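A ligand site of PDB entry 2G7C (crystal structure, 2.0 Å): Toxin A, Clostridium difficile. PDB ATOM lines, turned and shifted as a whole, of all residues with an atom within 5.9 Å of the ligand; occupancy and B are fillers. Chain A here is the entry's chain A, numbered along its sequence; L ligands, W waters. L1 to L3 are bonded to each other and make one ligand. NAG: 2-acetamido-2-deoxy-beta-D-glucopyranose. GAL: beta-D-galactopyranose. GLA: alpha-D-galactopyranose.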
ATOM      1  N   ASP A  54       5.878 -10.873  13.450  1.00  0.00           N
ATOM      2  CA  ASP A  54       6.919 -10.620  14.439  1.00  0.00           C
ATOM      3  C   ASP A  54       7.246  -9.152  14.687  1.00  0.00           C
ATOM      4  O   ASP A  54       8.353  -8.810  15.104  1.00  0.00           O
ATOM      5  CB  ASP A  54       8.187 -11.383  14.077  1.00  0.00           C
ATOM      6  CG  ASP A  54       8.003 -12.882  14.200  1.00  0.00           C
ATOM      7  OD1 ASP A  54       7.669 -13.340  15.310  1.00  0.00           O
ATOM      8  OD2 ASP A  54       8.183 -13.592  13.185  1.00  0.00           O
ATOM      9  N   LYS A  55       6.281  -8.292  14.416  1.00  0.00           N
ATOM     10  CA  LYS A  55       6.438  -6.870  14.648  1.00  0.00           C
ATOM     11  C   LYS A  55       5.227  -6.427  15.450  1.00  0.00           C
ATOM     12  O   LYS A  55       4.197  -7.091  15.433  1.00  0.00           O
ATOM     13  CB  LYS A  55       6.559  -6.098  13.337  1.00  0.00           C
ATOM     14  CG  LYS A  55       7.922  -6.278  12.684  1.00  0.00           C
ATOM     15  CD  LYS A  55       8.182  -5.227  11.616  1.00  0.00           C
ATOM     16  CE  LYS A  55       9.638  -5.274  11.156  1.00  0.00           C
ATOM     17  NZ  LYS A  55       9.980  -4.164  10.207  1.00  0.00           N
ATOM     18  N   HIS A  56       5.355  -5.313  16.154  1.00  0.00           N
ATOM     19  CA  HIS A  56       4.279  -4.800  16.999  1.00  0.00           C
ATOM     20  C   HIS A  56       3.564  -3.581  16.416  1.00  0.00           C
ATOM     21  O   HIS A  56       4.211  -2.648  15.949  1.00  0.00           O
ATOM     22  CB  HIS A  56       4.841  -4.414  18.363  1.00  0.00           C
ATOM     23  CG  HIS A  56       5.761  -5.450  18.961  1.00  0.00           C
ATOM     24  ND1 HIS A  56       6.573  -5.181  20.037  1.00  0.00           N
ATOM     25  CD2 HIS A  56       5.944  -6.758  18.655  1.00  0.00           C
ATOM     26  CE1 HIS A  56       7.238  -6.282  20.369  1.00  0.00           C
ATOM     27  NE2 HIS A  56       6.864  -7.246  19.552  1.00  0.00           N
ATOM     28  N   ASP A  74       4.452  -5.649  27.671  1.00  0.00           N
ATOM     29  CA  ASP A  74       5.789  -5.382  28.185  1.00  0.00           C
ATOM     30  C   ASP A  74       6.022  -3.895  28.469  1.00  0.00           C
ATOM     31  O   ASP A  74       7.162  -3.458  28.633  1.00  0.00           O
ATOM     32  CB  ASP A  74       6.853  -5.876  27.200  1.00  0.00           C
ATOM     33  CG  ASP A  74       6.803  -7.382  26.997  1.00  0.00           C
ATOM     34  OD1 ASP A  74       6.827  -8.113  28.005  1.00  0.00           O
ATOM     35  OD2 ASP A  74       6.744  -7.824  25.829  1.00  0.00           O
ATOM     36  N   PHE A  76       4.983   0.463  27.732  1.00  0.00           N
ATOM     37  CA  PHE A  76       4.641   1.381  26.657  1.00  0.00           C
ATOM     38  C   PHE A  76       5.686   1.356  25.554  1.00  0.00           C
ATOM     39  O   PHE A  76       6.874   1.554  25.811  1.00  0.00           O
ATOM     40  CB  PHE A  76       4.525   2.820  27.191  1.00  0.00           C
ATOM     41  CG  PHE A  76       3.314   3.060  28.050  1.00  0.00           C
ATOM     42  CD1 PHE A  76       3.336   2.746  29.400  1.00  0.00           C
ATOM     43  CD2 PHE A  76       2.181   3.661  27.504  1.00  0.00           C
ATOM     44  CE1 PHE A  76       2.228   3.014  30.214  1.00  0.00           C
ATOM     45  CE2 PHE A  76       1.067   3.932  28.306  1.00  0.00           C
ATOM     46  CZ  PHE A  76       1.089   3.619  29.655  1.00  0.00           C
ATOM     47  N   GLU A  77       5.230   1.105  24.331  1.00  0.00           N
ATOM     48  CA  GLU A  77       6.135   1.070  23.184  1.00  0.00           C
ATOM     49  C   GLU A  77       5.880   2.252  22.270  1.00  0.00           C
ATOM     50  O   GLU A  77       4.831   2.886  22.338  1.00  0.00           O
ATOM     51  CB  GLU A  77       5.949  -0.244  22.414  1.00  0.00           C
ATOM     52  CG  GLU A  77       6.206  -1.480  23.291  1.00  0.00           C
ATOM     53  CD  GLU A  77       6.210  -2.787  22.505  1.00  0.00           C
ATOM     54  OE1 GLU A  77       6.512  -2.758  21.301  1.00  0.00           O
ATOM     55  OE2 GLU A  77       5.942  -3.839  23.106  1.00  0.00           O
ATOM     56  N   TYR A  78       6.853   2.550  21.417  1.00  0.00           N
ATOM     57  CA  TYR A  78       6.718   3.660  20.491  1.00  0.00           C
ATOM     58  C   TYR A  78       6.407   3.146  19.094  1.00  0.00           C
ATOM     59  O   TYR A  78       7.276   2.579  18.428  1.00  0.00           O
ATOM     60  CB  TYR A  78       8.008   4.491  20.465  1.00  0.00           C
ATOM     61  CG  TYR A  78       7.994   5.662  19.501  1.00  0.00           C
ATOM     62  CD1 TYR A  78       6.794   6.265  19.109  1.00  0.00           C
ATOM     63  CD2 TYR A  78       9.189   6.203  19.006  1.00  0.00           C
ATOM     64  CE1 TYR A  78       6.781   7.376  18.258  1.00  0.00           C
ATOM     65  CE2 TYR A  78       9.182   7.308  18.150  1.00  0.00           C
ATOM     66  CZ  TYR A  78       7.983   7.878  17.782  1.00  0.00           C
ATOM     67  OH  TYR A  78       7.973   8.980  16.950  1.00  0.00           O
ATOM     68  N   ASP A  85      13.667   4.526  12.526  1.00  0.00           N
ATOM     69  CA  ASP A  85      14.825   3.759  12.947  1.00  0.00           C
ATOM     70  C   ASP A  85      14.961   2.540  12.053  1.00  0.00           C
ATOM     71  O   ASP A  85      14.039   1.728  11.950  1.00  0.00           O
ATOM     72  CB  ASP A  85      14.672   3.309  14.405  1.00  0.00           C
ATOM     73  CG  ASP A  85      15.896   2.562  14.904  1.00  0.00           C
ATOM     74  OD1 ASP A  85      16.956   3.196  15.082  1.00  0.00           O
ATOM     75  OD2 ASP A  85      15.801   1.332  15.110  1.00  0.00           O
ATOM     76  N   ALA A  86      16.104   2.420  11.389  1.00  0.00           N
ATOM     77  CA  ALA A  86      16.353   1.292  10.498  1.00  0.00           C
ATOM     78  C   ALA A  86      15.189   1.098   9.534  1.00  0.00           C
ATOM     79  O   ALA A  86      14.672  -0.015   9.397  1.00  0.00           O
ATOM     80  CB  ALA A  86      16.578   0.029  11.313  1.00  0.00           C
ATOM     81  N   ASN A  88      11.997   1.537   9.551  1.00  0.00           N
ATOM     82  CA  ASN A  88      10.886   0.755  10.077  1.00  0.00           C
ATOM     83  C   ASN A  88       9.627   1.126   9.307  1.00  0.00           C
ATOM     84  O   ASN A  88       9.524   2.245   8.778  1.00  0.00           O
ATOM     85  CB  ASN A  88      10.651   1.075  11.548  1.00  0.00           C
ATOM     86  CG  ASN A  88      10.266   2.517  11.765  1.00  0.00           C
ATOM     87  OD1 ASN A  88      11.127   3.397  11.792  1.00  0.00           O
ATOM     88  ND2 ASN A  88       8.963   2.780  11.893  1.00  0.00           N
ATOM     89  N   GLN A  92       4.810   0.572  13.175  1.00  0.00           N
ATOM     90  CA  GLN A  92       5.567  -0.485  13.854  1.00  0.00           C
ATOM     91  C   GLN A  92       6.244   0.068  15.111  1.00  0.00           C
ATOM     92  O   GLN A  92       6.641   1.229  15.153  1.00  0.00           O
ATOM     93  CB  GLN A  92       6.645  -1.005  12.904  1.00  0.00           C
ATOM     94  CG  GLN A  92       7.608  -1.970  13.538  1.00  0.00           C
ATOM     95  CD  GLN A  92       8.962  -1.944  12.855  1.00  0.00           C
ATOM     96  OE1 GLN A  92       9.062  -1.889  11.625  1.00  0.00           O
ATOM     97  NE2 GLN A  92      10.030  -1.987  13.652  1.00  0.00           N
ATOM     98  N   ALA A  93       6.343  -0.766  16.151  1.00  0.00           N
ATOM     99  CA  ALA A  93       7.009  -0.355  17.382  1.00  0.00           C
ATOM    100  C   ALA A  93       8.491  -0.469  17.061  1.00  0.00           C
ATOM    101  O   ALA A  93       8.923  -1.444  16.430  1.00  0.00           O
ATOM    102  CB  ALA A  93       6.645  -1.281  18.529  1.00  0.00           C
ATOM    103  N   ILE A  94       9.278   0.501  17.507  1.00  0.00           N
ATOM    104  CA  ILE A  94      10.709   0.486  17.198  1.00  0.00           C
ATOM    105  C   ILE A  94      11.654   0.524  18.394  1.00  0.00           C
ATOM    106  O   ILE A  94      11.242   0.779  19.534  1.00  0.00           O
ATOM    107  CB  ILE A  94      11.079   1.683  16.310  1.00  0.00           C
ATOM    108  CG1 ILE A  94      10.812   2.992  17.076  1.00  0.00           C
ATOM    109  CG2 ILE A  94      10.280   1.640  15.020  1.00  0.00           C
ATOM    110  CD1 ILE A  94      11.251   4.236  16.350  1.00  0.00           C
ATOM    111  N   ARG A  95      12.917   0.264  18.103  1.00  0.00           N
ATOM    112  CA  ARG A  95      13.965   0.330  19.112  1.00  0.00           C
ATOM    113  C   ARG A  95      14.144   1.831  19.313  1.00  0.00           C
ATOM    114  O   ARG A  95      14.362   2.581  18.355  1.00  0.00           O
ATOM    115  CB  ARG A  95      15.277  -0.262  18.572  1.00  0.00           C
ATOM    116  CG  ARG A  95      16.354  -0.454  19.623  1.00  0.00           C
ATOM    117  CD  ARG A  95      17.724  -0.526  18.990  1.00  0.00           C
ATOM    118  NE  ARG A  95      18.070   0.767  18.401  1.00  0.00           N
ATOM    119  CZ  ARG A  95      19.202   1.017  17.752  1.00  0.00           C
ATOM    120  NH1 ARG A  95      20.110   0.055  17.602  1.00  0.00           N
ATOM    121  NH2 ARG A  95      19.431   2.217  17.254  1.00  0.00           N
ATOM    122  N   TYR A  96      14.029   2.271  20.563  1.00  0.00           N
ATOM    123  CA  TYR A  96      14.176   3.686  20.885  1.00  0.00           C
ATOM    124  C   TYR A  96      14.691   3.602  22.309  1.00  0.00           C
ATOM    125  O   TYR A  96      13.922   3.387  23.250  1.00  0.00           O
ATOM    126  CB  TYR A  96      12.801   4.359  20.826  1.00  0.00           C
ATOM    127  CG  TYR A  96      12.857   5.873  20.714  1.00  0.00           C
ATOM    128  CD1 TYR A  96      13.189   6.495  19.507  1.00  0.00           C
ATOM    129  CD2 TYR A  96      12.617   6.682  21.823  1.00  0.00           C
ATOM    130  CE1 TYR A  96      13.274   7.878  19.417  1.00  0.00           C
ATOM    131  CE2 TYR A  96      12.699   8.058  21.740  1.00  0.00           C
ATOM    132  CZ  TYR A  96      13.033   8.653  20.550  1.00  0.00           C
ATOM    133  OH  TYR A  96      13.162  10.024  20.502  1.00  0.00           O
ATOM    134  N   GLN A  97      16.006   3.755  22.454  1.00  0.00           N
ATOM    135  CA  GLN A  97      16.640   3.611  23.751  1.00  0.00           C
ATOM    136  C   GLN A  97      17.233   4.845  24.431  1.00  0.00           C
ATOM    137  O   GLN A  97      17.798   5.729  23.785  1.00  0.00           O
ATOM    138  CB  GLN A  97      17.753   2.571  23.662  1.00  0.00           C
ATOM    139  CG  GLN A  97      17.349   1.211  23.133  1.00  0.00           C
ATOM    140  CD  GLN A  97      18.554   0.340  22.876  1.00  0.00           C
ATOM    141  OE1 GLN A  97      19.233   0.472  21.862  1.00  0.00           O
ATOM    142  NE2 GLN A  97      18.841  -0.561  23.813  1.00  0.00           N
ATOM    143  N   GLY A 111      13.462   4.062  28.210  1.00  0.00           N
ATOM    144  CA  GLY A 111      14.584   3.399  28.849  1.00  0.00           C
ATOM    145  C   GLY A 111      15.439   2.551  27.924  1.00  0.00           C
ATOM    146  O   GLY A 111      15.312   2.628  26.702  1.00  0.00           O
ATOM    147  N   ASN A 112      16.312   1.728  28.518  1.00  0.00           N
ATOM    148  CA  ASN A 112      17.199   0.864  27.740  1.00  0.00           C
ATOM    149  C   ASN A 112      16.415  -0.237  27.014  1.00  0.00           C
ATOM    150  O   ASN A 112      16.868  -0.758  25.994  1.00  0.00           O
ATOM    151  CB  ASN A 112      18.254   0.241  28.668  1.00  0.00           C
ATOM    152  CG  ASN A 112      19.374  -0.454  27.897  1.00  0.00           C
ATOM    153  OD1 ASN A 112      19.698  -1.614  28.174  1.00  0.00           O
ATOM    154  ND2 ASN A 112      19.986   0.258  26.959  1.00  0.00           N
ATOM    155  N   ASN A 113      15.234  -0.567  27.533  1.00  0.00           N
ATOM    156  CA  ASN A 113      14.379  -1.607  26.961  1.00  0.00           C
ATOM    157  C   ASN A 113      13.407  -1.097  25.902  1.00  0.00           C
ATOM    158  O   ASN A 113      12.481  -1.808  25.501  1.00  0.00           O
ATOM    159  CB  ASN A 113      13.574  -2.276  28.077  1.00  0.00           C
ATOM    160  CG  ASN A 113      12.748  -1.285  28.864  1.00  0.00           C
ATOM    161  OD1 ASN A 113      12.732  -0.097  28.563  1.00  0.00           O
ATOM    162  ND2 ASN A 113      12.051  -1.767  29.904  1.00  0.00           N
ATOM    163  N   SER A 114      13.617   0.141  25.438  1.00  0.00           N
ATOM    164  CA  SER A 114      12.747   0.750  24.444  1.00  0.00           C
ATOM    165  C   SER A 114      11.322   0.897  24.951  1.00  0.00           C
ATOM    166  O   SER A 114      10.374   0.982  24.167  1.00  0.00           O
ATOM    167  CB  SER A 114      12.747  -0.072  23.137  1.00  0.00           C
ATOM    168  OG  SER A 114      13.988   0.031  22.472  1.00  0.00           O
ATOM    169  N   LYS A 115      11.152   0.920  26.268  1.00  0.00           N
ATOM    170  CA  LYS A 115       9.825   1.097  26.842  1.00  0.00           C
ATOM    171  C   LYS A 115       9.818   2.460  27.540  1.00  0.00           C
ATOM    172  O   LYS A 115      10.844   2.876  28.077  1.00  0.00           O
ATOM    173  CB  LYS A 115       9.534  -0.018  27.854  1.00  0.00           C
ATOM    174  CG  LYS A 115       9.642  -1.438  27.281  1.00  0.00           C
ATOM    175  CD  LYS A 115       8.595  -1.709  26.188  1.00  0.00           C
ATOM    176  CE  LYS A 115       8.776  -3.103  25.574  1.00  0.00           C
ATOM    177  NZ  LYS A 115      10.035  -3.216  24.776  1.00  0.00           N
HETATM  178  C1  NAG L   1      15.191  -5.038  25.746  1.00  0.00           C
HETATM  179  C2  NAG L   1      13.681  -5.175  25.554  1.00  0.00           C
HETATM  180  C3  NAG L   1      13.355  -5.276  24.056  1.00  0.00           C
HETATM  181  C4  NAG L   1      14.016  -4.132  23.260  1.00  0.00           C
HETATM  182  C5  NAG L   1      15.504  -4.040  23.601  1.00  0.00           C
HETATM  183  C6  NAG L   1      16.170  -2.841  22.972  1.00  0.00           C
HETATM  184  C7  NAG L   1      11.997  -6.343  26.821  1.00  0.00           C
HETATM  185  C8  NAG L   1      11.389  -7.705  27.139  1.00  0.00           C
HETATM  186  N2  NAG L   1      13.205  -6.346  26.257  1.00  0.00           N
HETATM  187  O1  NAG L   1      15.480  -4.855  27.089  1.00  0.00           O
HETATM  188  O3  NAG L   1      11.953  -5.225  23.859  1.00  0.00           O
HETATM  189  O4  NAG L   1      13.871  -4.406  21.852  1.00  0.00           O
HETATM  190  O5  NAG L   1      15.677  -3.907  25.022  1.00  0.00           O
HETATM  191  O6  NAG L   1      15.714  -1.631  23.554  1.00  0.00           O
HETATM  192  O7  NAG L   1      11.381  -5.310  27.096  1.00  0.00           O
HETATM  193  C1  GAL L   2      13.198  -3.490  21.060  1.00  0.00           C
HETATM  194  C2  GAL L   2      13.355  -3.937  19.602  1.00  0.00           C
HETATM  195  C3  GAL L   2      12.359  -3.296  18.622  1.00  0.00           C
HETATM  196  C4  GAL L   2      10.951  -3.307  19.222  1.00  0.00           C
HETATM  197  C5  GAL L   2      10.983  -2.702  20.609  1.00  0.00           C
HETATM  198  C6  GAL L   2       9.604  -2.641  21.243  1.00  0.00           C
HETATM  199  O2  GAL L   2      14.674  -3.638  19.158  1.00  0.00           O
HETATM  200  O3  GAL L   2      12.395  -4.064  17.390  1.00  0.00           O
HETATM  201  O4  GAL L   2      10.506  -4.650  19.318  1.00  0.00           O
HETATM  202  O5  GAL L   2      11.809  -3.518  21.452  1.00  0.00           O
HETATM  203  O6  GAL L   2       9.589  -1.758  22.366  1.00  0.00           O
HETATM  204  C1  GLA L   3      11.581  -3.657  16.328  1.00  0.00           C
HETATM  205  C2  GLA L   3      11.524  -4.784  15.278  1.00  0.00           C
HETATM  206  C3  GLA L   3      12.887  -4.931  14.601  1.00  0.00           C
HETATM  207  C4  GLA L   3      13.319  -3.600  13.998  1.00  0.00           C
HETATM  208  C5  GLA L   3      13.312  -2.509  15.069  1.00  0.00           C
HETATM  209  C6  GLA L   3      13.569  -1.134  14.480  1.00  0.00           C
HETATM  210  O2  GLA L   3      11.183  -6.010  15.919  1.00  0.00           O
HETATM  211  O3  GLA L   3      12.813  -5.912  13.573  1.00  0.00           O
HETATM  212  O4  GLA L   3      12.453  -3.262  12.928  1.00  0.00           O
HETATM  213  O5  GLA L   3      12.019  -2.443  15.714  1.00  0.00           O
HETATM  214  O6  GLA L   3      13.675  -0.143  15.496  1.00  0.00           O
HETATM  215  O   HOH W   1       8.920  -6.048  17.239  1.00  0.00           O
HETATM  216  O   HOH W   2       9.232   0.802  21.551  1.00  0.00           O
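The side-chain carboxylate (OD2) of Asp 85 lies within hydrogen-bond range of an oxygen (O6) of GLA L3 (2.6 Å).
O6 of NAG L1 lies within hydrogen-bond range of N of Ser 114, at 3.3 Å.
The backbone carbonyl oxygen (O) of Ser 114 sits at hydrogen-bond distance from an oxygen (O6) of GAL L2, at 3.4 Å.
OG of Ser 114 is in hydrogen-bond range of O6 of NAG L1 (2.6 Å).
O6 of GLA L3 sits at hydrogen-bond distance from N of Arg 95, 2.7 Å away.
O4 of GLA L3 is in hydrogen-bond range of NE2 of Gln 92.
O of Asn 112 lies within hydrogen-bond range of O6 of NAG L1, at 2.8 Å.
NZ of Lys 115 sits at hydrogen-bond distance from O6 of GAL L2 (2.9 Å).
OE1 of Glu 77 lies close to O6 of GAL L2.
NE2 of Gln 97 lies close to O6 of NAG L1 (3.3 Å).
OD1 of Asp 85 is in salt-bridge range of NH2 of Arg 95 (3.4 Å).
OD1 of Asn 88 is in hydrogen-bond range of N of Asp 85, 2.9 Å away.
OG of Ser 114 lies within hydrogen-bond range of N of Tyr 96, at 2.9 Å.
OE1 of Gln 92 is in hydrogen-bond range of NZ of Lys 55 (2.8 Å).
O of Asn 112 is in hydrogen-bond range of NE2 of Gln 97, at 2.9 Å.
ND1 of His 56 sits at hydrogen-bond distance from OE1 of Glu 77, 2.7 Å away.
N of Ile 94 is in hydrogen-bond range of O of Tyr 78 (3.0 Å).
The backbone NH of Ala 93 lies within hydrogen-bond range of the backbone carbonyl oxygen of His 56, at 2.9 Å.
O5 of GLA L3 sits close to O of Ala 93 (3.3 Å).
Residues that only touch the ligand: Asn 113 (3.3 Å), Ile 94 (3.3 Å), Lys 55 (3.8 Å) and His 56 (3.8 Å).
Hydrophobic or aromatic side chains that line the ligand: His 56 and Ile 94.
13 residues have an atom within 4 Å of the ligand: Lys 55, His 56, Glu 77, Asp 85, Gln 92, Ala 93, Ile 94, Arg 95, Gln 97, Asn 112, Asn 113, Ser 114 and Lys 115.
The nearest printed residue that does not touch the ligand is Asp 54 (4.1 Å).
Water W1 bridges an oxygen (O2) of GLA L3 and a ring nitrogen (NE2) of His 56.
Water W2 lies within hydrogen-bond range of O6 of GAL L2 (2.7 Å), O of Ile 94 (2.8 Å), O of Ser 114 (2.9 Å) and N of Tyr 78 (3.0 Å).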
